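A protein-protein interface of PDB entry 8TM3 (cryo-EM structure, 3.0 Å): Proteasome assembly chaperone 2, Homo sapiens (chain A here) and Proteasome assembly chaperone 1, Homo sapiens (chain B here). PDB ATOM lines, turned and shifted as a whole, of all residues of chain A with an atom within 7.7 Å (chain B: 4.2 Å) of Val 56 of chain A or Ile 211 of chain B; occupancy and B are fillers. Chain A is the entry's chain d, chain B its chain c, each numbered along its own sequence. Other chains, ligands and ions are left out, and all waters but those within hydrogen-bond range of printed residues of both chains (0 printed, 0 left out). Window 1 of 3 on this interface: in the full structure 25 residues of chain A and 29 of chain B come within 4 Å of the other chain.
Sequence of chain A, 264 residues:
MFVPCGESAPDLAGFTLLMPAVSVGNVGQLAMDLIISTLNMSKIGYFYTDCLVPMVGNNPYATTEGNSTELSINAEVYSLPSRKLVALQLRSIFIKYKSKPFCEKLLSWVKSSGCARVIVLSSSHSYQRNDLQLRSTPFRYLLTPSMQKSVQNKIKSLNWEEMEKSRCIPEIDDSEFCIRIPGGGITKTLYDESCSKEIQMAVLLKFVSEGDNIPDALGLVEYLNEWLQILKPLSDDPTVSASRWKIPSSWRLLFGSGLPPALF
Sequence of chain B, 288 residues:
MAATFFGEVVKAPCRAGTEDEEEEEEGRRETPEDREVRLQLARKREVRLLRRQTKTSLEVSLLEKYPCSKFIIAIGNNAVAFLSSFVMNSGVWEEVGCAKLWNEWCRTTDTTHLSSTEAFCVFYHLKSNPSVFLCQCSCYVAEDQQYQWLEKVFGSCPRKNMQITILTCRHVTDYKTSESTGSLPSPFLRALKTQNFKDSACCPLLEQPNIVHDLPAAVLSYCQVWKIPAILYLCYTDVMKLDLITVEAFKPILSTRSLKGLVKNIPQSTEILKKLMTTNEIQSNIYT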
ATOM      1  N   VAL A  53       6.307 -22.101  -6.371  1.00  0.00           N
ATOM      2  CA  VAL A  53       7.713 -21.727  -6.564  1.00  0.00           C
ATOM      3  C   VAL A  53       7.787 -20.596  -7.587  1.00  0.00           C
ATOM      4  O   VAL A  53       7.195 -20.710  -8.676  1.00  0.00           O
ATOM      5  CB  VAL A  53       8.541 -22.940  -7.008  1.00  0.00           C
ATOM      6  CG1 VAL A  53       8.167 -24.177  -6.202  1.00  0.00           C
ATOM      7  CG2 VAL A  53       8.378 -23.210  -8.499  1.00  0.00           C
ATOM      8  N   PRO A  54       8.470 -19.494  -7.290  1.00  0.00           N
ATOM      9  CA  PRO A  54       8.447 -18.350  -8.207  1.00  0.00           C
ATOM     10  C   PRO A  54       9.063 -18.678  -9.557  1.00  0.00           C
ATOM     11  O   PRO A  54      10.013 -19.456  -9.667  1.00  0.00           O
ATOM     12  CB  PRO A  54       9.266 -17.285  -7.468  1.00  0.00           C
ATOM     13  CG  PRO A  54      10.093 -18.037  -6.490  1.00  0.00           C
ATOM     14  CD  PRO A  54       9.303 -19.239  -6.103  1.00  0.00           C
ATOM     15  N   MET A  55       8.497 -18.068 -10.596  1.00  0.00           N
ATOM     16  CA  MET A  55       9.038 -18.159 -11.943  1.00  0.00           C
ATOM     17  C   MET A  55       8.661 -16.894 -12.697  1.00  0.00           C
ATOM     18  O   MET A  55       7.653 -16.253 -12.393  1.00  0.00           O
ATOM     19  CB  MET A  55       8.520 -19.396 -12.688  1.00  0.00           C
ATOM     20  CG  MET A  55       7.002 -19.513 -12.735  1.00  0.00           C
ATOM     21  SD  MET A  55       6.227 -18.544 -14.046  1.00  0.00           S
ATOM     22  CE  MET A  55       6.990 -19.230 -15.513  1.00  0.00           C
ATOM     23  N   VAL A  56       9.482 -16.538 -13.687  1.00  0.00           N
ATOM     24  CA  VAL A  56       9.261 -15.343 -14.490  1.00  0.00           C
ATOM     25  C   VAL A  56       9.529 -15.661 -15.954  1.00  0.00           C
ATOM     26  O   VAL A  56      10.217 -16.626 -16.292  1.00  0.00           O
ATOM     27  CB  VAL A  56      10.145 -14.161 -14.038  1.00  0.00           C
ATOM     28  CG1 VAL A  56       9.588 -13.544 -12.767  1.00  0.00           C
ATOM     29  CG2 VAL A  56      11.583 -14.615 -13.838  1.00  0.00           C
ATOM     30  N   GLY A  57       8.974 -14.826 -16.823  1.00  0.00           N
ATOM     31  CA  GLY A  57       9.167 -14.983 -18.252  1.00  0.00           C
ATOM     32  C   GLY A  57       8.373 -13.932 -18.994  1.00  0.00           C
ATOM     33  O   GLY A  57       7.553 -13.211 -18.413  1.00  0.00           O
ATOM     34  N   ASN A  58       8.624 -13.859 -20.297  1.00  0.00           N
ATOM     35  CA  ASN A  58       7.928 -12.900 -21.141  1.00  0.00           C
ATOM     36  C   ASN A  58       6.445 -13.258 -21.216  1.00  0.00           C
ATOM     37  O   ASN A  58       5.981 -14.244 -20.635  1.00  0.00           O
ATOM     38  CB  ASN A  58       8.561 -12.864 -22.530  1.00  0.00           C
ATOM     39  CG  ASN A  58       9.734 -11.908 -22.610  1.00  0.00           C
ATOM     40  OD1 ASN A  58      10.161 -11.344 -21.603  1.00  0.00           O
ATOM     41  ND2 ASN A  58      10.263 -11.721 -23.813  1.00  0.00           N
ATOM     42  N   GLU A  70       6.792  -8.416 -21.978  1.00  0.00           N
ATOM     43  CA  GLU A  70       6.102  -8.261 -20.706  1.00  0.00           C
ATOM     44  C   GLU A  70       6.757  -9.198 -19.697  1.00  0.00           C
ATOM     45  O   GLU A  70       7.833  -9.751 -19.942  1.00  0.00           O
ATOM     46  CB  GLU A  70       4.601  -8.535 -20.865  1.00  0.00           C
ATOM     47  N   LEU A  71       6.105  -9.371 -18.550  1.00  0.00           N
ATOM     48  CA  LEU A  71       6.600 -10.236 -17.486  1.00  0.00           C
ATOM     49  C   LEU A  71       5.446 -11.088 -16.983  1.00  0.00           C
ATOM     50  O   LEU A  71       4.359 -10.568 -16.717  1.00  0.00           O
ATOM     51  CB  LEU A  71       7.203  -9.412 -16.347  1.00  0.00           C
ATOM     52  CG  LEU A  71       8.248 -10.109 -15.474  1.00  0.00           C
ATOM     53  CD1 LEU A  71       9.461 -10.517 -16.293  1.00  0.00           C
ATOM     54  CD2 LEU A  71       8.658  -9.204 -14.330  1.00  0.00           C
ATOM     55  N   SER A  72       5.682 -12.393 -16.856  1.00  0.00           N
ATOM     56  CA  SER A  72       4.660 -13.350 -16.445  1.00  0.00           C
ATOM     57  C   SER A  72       5.139 -14.073 -15.193  1.00  0.00           C
ATOM     58  O   SER A  72       6.015 -14.940 -15.269  1.00  0.00           O
ATOM     59  CB  SER A  72       4.358 -14.341 -17.568  1.00  0.00           C
ATOM     60  N   ILE A  73       4.559 -13.720 -14.048  1.00  0.00           N
ATOM     61  CA  ILE A  73       4.913 -14.337 -12.773  1.00  0.00           C
ATOM     62  C   ILE A  73       4.178 -15.662 -12.623  1.00  0.00           C
ATOM     63  O   ILE A  73       3.294 -15.991 -13.421  1.00  0.00           O
ATOM     64  CB  ILE A  73       4.606 -13.406 -11.587  1.00  0.00           C
ATOM     65  CG1 ILE A  73       3.125 -13.024 -11.570  1.00  0.00           C
ATOM     66  CG2 ILE A  73       5.486 -12.167 -11.652  1.00  0.00           C
ATOM     67  CD1 ILE A  73       2.768 -12.035 -10.493  1.00  0.00           C
ATOM     68  N   ASN A  74       4.550 -16.432 -11.596  1.00  0.00           N
ATOM     69  CA  ASN A  74       3.977 -17.760 -11.404  1.00  0.00           C
ATOM     70  C   ASN A  74       2.455 -17.730 -11.356  1.00  0.00           C
ATOM     71  O   ASN A  74       1.804 -18.660 -11.845  1.00  0.00           O
ATOM     72  CB  ASN A  74       4.527 -18.378 -10.119  1.00  0.00           C
ATOM     73  CG  ASN A  74       4.186 -17.562  -8.892  1.00  0.00           C
ATOM     74  OD1 ASN A  74       3.640 -16.465  -8.995  1.00  0.00           O
ATOM     75  ND2 ASN A  74       4.514 -18.091  -7.720  1.00  0.00           N
ATOM     76  N   ARG A  91       0.920 -21.408 -13.397  1.00  0.00           N
ATOM     77  CA  ARG A  91       2.014 -21.817 -14.267  1.00  0.00           C
ATOM     78  C   ARG A  91       3.226 -22.255 -13.454  1.00  0.00           C
ATOM     79  O   ARG A  91       4.370 -22.076 -13.890  1.00  0.00           O
ATOM     80  CB  ARG A  91       2.401 -20.688 -15.229  1.00  0.00           C
ATOM     81  CG  ARG A  91       2.233 -19.288 -14.652  1.00  0.00           C
ATOM     82  CD  ARG A  91       2.457 -18.216 -15.704  1.00  0.00           C
ATOM     83  NE  ARG A  91       1.396 -18.202 -16.707  1.00  0.00           N
ATOM     84  CZ  ARG A  91       1.575 -18.397 -18.008  1.00  0.00           C
ATOM     85  NH1 ARG A  91       2.772 -18.631 -18.518  1.00  0.00           N
ATOM     86  NH2 ARG A  91       0.523 -18.359 -18.818  1.00  0.00           N
ATOM     87  N   SER A  92       3.000 -22.832 -12.276  1.00  0.00           N
ATOM     88  CA  SER A  92       4.087 -23.188 -11.377  1.00  0.00           C
ATOM     89  C   SER A  92       3.733 -24.445 -10.598  1.00  0.00           C
ATOM     90  O   SER A  92       2.562 -24.794 -10.434  1.00  0.00           O
ATOM     91  CB  SER A  92       4.403 -22.043 -10.408  1.00  0.00           C
ATOM     92  OG  SER A  92       5.340 -22.452  -9.429  1.00  0.00           O
ATOM     93  N   ASP B 174      19.498 -25.013 -19.966  1.00  0.00           N
ATOM     94  CA  ASP B 174      18.245 -24.390 -19.556  1.00  0.00           C
ATOM     95  C   ASP B 174      17.655 -23.544 -20.675  1.00  0.00           C
ATOM     96  O   ASP B 174      16.429 -23.439 -20.791  1.00  0.00           O
ATOM     97  CB  ASP B 174      18.472 -23.543 -18.303  1.00  0.00           C
ATOM     98  CG  ASP B 174      17.323 -22.587 -18.021  1.00  0.00           C
ATOM     99  OD1 ASP B 174      17.134 -21.622 -18.792  1.00  0.00           O
ATOM    100  OD2 ASP B 174      16.608 -22.801 -17.020  1.00  0.00           O
ATOM    101  N   PRO B 209       9.165 -18.927 -24.814  1.00  0.00           N
ATOM    102  CA  PRO B 209       9.077 -20.199 -24.078  1.00  0.00           C
ATOM    103  C   PRO B 209      10.068 -20.313 -22.937  1.00  0.00           C
ATOM    104  O   PRO B 209       9.860 -21.137 -22.037  1.00  0.00           O
ATOM    105  CB  PRO B 209       9.347 -21.250 -25.162  1.00  0.00           C
ATOM    106  CG  PRO B 209      10.183 -20.547 -26.158  1.00  0.00           C
ATOM    107  CD  PRO B 209       9.712 -19.119 -26.169  1.00  0.00           C
ATOM    108  N   ASN B 210      11.136 -19.521 -22.940  1.00  0.00           N
ATOM    109  CA  ASN B 210      12.157 -19.623 -21.910  1.00  0.00           C
ATOM    110  C   ASN B 210      11.671 -18.961 -20.628  1.00  0.00           C
ATOM    111  O   ASN B 210      11.012 -17.917 -20.669  1.00  0.00           O
ATOM    112  CB  ASN B 210      13.451 -18.968 -22.385  1.00  0.00           C
ATOM    113  CG  ASN B 210      13.855 -19.428 -23.767  1.00  0.00           C
ATOM    114  OD1 ASN B 210      13.085 -20.086 -24.463  1.00  0.00           O
ATOM    115  ND2 ASN B 210      15.069 -19.093 -24.170  1.00  0.00           N
ATOM    116  N   ILE B 211      11.992 -19.573 -19.487  1.00  0.00           N
ATOM    117  CA  ILE B 211      11.583 -19.065 -18.187  1.00  0.00           C
ATOM    118  C   ILE B 211      12.762 -19.150 -17.228  1.00  0.00           C
ATOM    119  O   ILE B 211      13.771 -19.804 -17.497  1.00  0.00           O
ATOM    120  CB  ILE B 211      10.356 -19.825 -17.624  1.00  0.00           C
ATOM    121  CG1 ILE B 211      10.759 -21.113 -16.893  1.00  0.00           C
ATOM    122  CG2 ILE B 211       9.385 -20.159 -18.742  1.00  0.00           C
ATOM    123  CD1 ILE B 211       9.641 -21.700 -16.073  1.00  0.00           C
ATOM    124  N   VAL B 212      12.618 -18.470 -16.093  1.00  0.00           N
ATOM    125  CA  VAL B 212      13.607 -18.488 -15.024  1.00  0.00           C
ATOM    126  C   VAL B 212      12.883 -18.706 -13.705  1.00  0.00           C
ATOM    127  O   VAL B 212      11.830 -18.107 -13.459  1.00  0.00           O
ATOM    128  CB  VAL B 212      14.429 -17.184 -14.984  1.00  0.00           C
ATOM    129  CG1 VAL B 212      15.525 -17.282 -13.935  1.00  0.00           C
ATOM    130  CG2 VAL B 212      15.019 -16.887 -16.351  1.00  0.00           C
ATOM    131  N   ALA B 217      14.092 -15.305  -9.884  1.00  0.00           N
ATOM    132  CA  ALA B 217      12.684 -15.194 -10.234  1.00  0.00           C
ATOM    133  C   ALA B 217      11.859 -14.712  -9.051  1.00  0.00           C
ATOM    134  O   ALA B 217      10.910 -13.947  -9.237  1.00  0.00           O
ATOM    135  CB  ALA B 217      12.160 -16.539 -10.734  1.00  0.00           C
ATOM    136  N   LEU B 220      12.416 -10.961  -8.794  1.00  0.00           N
ATOM    137  CA  LEU B 220      11.792 -10.281  -9.923  1.00  0.00           C
ATOM    138  C   LEU B 220      10.273 -10.273  -9.793  1.00  0.00           C
ATOM    139  O   LEU B 220       9.622  -9.274 -10.116  1.00  0.00           O
ATOM    140  CB  LEU B 220      12.221 -10.938 -11.233  1.00  0.00           C
ATOM    141  CG  LEU B 220      12.200 -10.018 -12.454  1.00  0.00           C
ATOM    142  CD1 LEU B 220      13.315  -8.989 -12.369  1.00  0.00           C
ATOM    143  CD2 LEU B 220      12.316 -10.823 -13.735  1.00  0.00           C
ATOM    144  N   SER B 221       9.687 -11.376  -9.325  1.00  0.00           N
ATOM    145  CA  SER B 221       8.247 -11.409  -9.105  1.00  0.00           C
ATOM    146  C   SER B 221       7.838 -10.424  -8.019  1.00  0.00           C
ATOM    147  O   SER B 221       6.828  -9.724  -8.153  1.00  0.00           O
ATOM    148  CB  SER B 221       7.803 -12.826  -8.740  1.00  0.00           C
ATOM    149  OG  SER B 221       7.656 -12.969  -7.337  1.00  0.00           O
ATOM    150  N   LEU B 232      16.540  -8.450 -14.759  1.00  0.00           N
ATOM    151  CA  LEU B 232      17.161  -9.718 -14.392  1.00  0.00           C
ATOM    152  C   LEU B 232      18.044 -10.169 -15.549  1.00  0.00           C
ATOM    153  O   LEU B 232      17.542 -10.511 -16.625  1.00  0.00           O
ATOM    154  CB  LEU B 232      16.094 -10.759 -14.060  1.00  0.00           C
ATOM    155  CG  LEU B 232      16.506 -12.231 -13.991  1.00  0.00           C
ATOM    156  CD1 LEU B 232      17.766 -12.420 -13.166  1.00  0.00           C
ATOM    157  CD2 LEU B 232      15.369 -13.072 -13.430  1.00  0.00           C
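Val 56 of chain A touches just these residues of chain B: Ile 211, Val 212, Ala 217 and Leu 220.
Glu 70 of chain A touches none of the printed residues of chain B.
Printed residues of chain B within 4 Å of Ile 73 of chain A: Ser 221.
Ile 211 of chain B touches just these residues of chain A: Met 55 and Val 56.
Of the printed residues of chain A, Val 212 of chain B touches Met 55 (3.2 Å) and Val 56 (2.8 Å).
Printed residues of chain A within 4 Å of Ala 217 of chain B: Pro 54, Met 55 and Val 56.
Of the printed residues of chain A, Ser 221 of chain B touches Ile 73 (3.8 Å).
Among the printed residues, pairs that only touch across the chains: Pro 54 of chain A with Ala 217 of chain B (3.8 Å), Met 55 of chain A with Ile 211 of chain B (3.7 Å), Met 55 of chain A with Val 212 of chain B (3.2 Å), Met 55 of chain A with Ala 217 of chain B (3.7 Å), Val 56 of chain A with Ile 211 of chain B (3.4 Å), Val 56 of chain A with Ala 217 of chain B (3.7 Å), Val 56 of chain A with Leu 220 of chain B (3.9 Å), Leu 71 of chain A with Leu 220 of chain B (3.8 Å) and Ile 73 of chain A with Ser 221 of chain B (3.8 Å).
O of Met 55 of chain A is in hydrogen-bond range of N of Asn 74 of chain A (3.2 Å).
Of the 9 printed residues of chain B, 5 touch a printed residue of chain A.
Hydrophobic or aromatic side chains of chain B within 4 Å of the printed part of chain A: Ile 211, Ala 217 and Leu 220.
Of the 13 printed residues of chain A, 5 touch a printed residue of chain B.
Hydrophobic or aromatic side chains of chain A that line the printed part of chain B: Pro 54, Met 55, Val 56, Leu 71 and Ile 73.
Among the printed residues, 10 pairs touch across the chains.
Among the printed residues, no Asp or Glu carboxylate lies within 4 Å of a Lys or Arg side-chain nitrogen of the other chain.
The backbone carbonyl oxygen of Val 212 of chain B lies within hydrogen-bond range of the backbone NH of Val 56 of chain A (2.8 Å).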
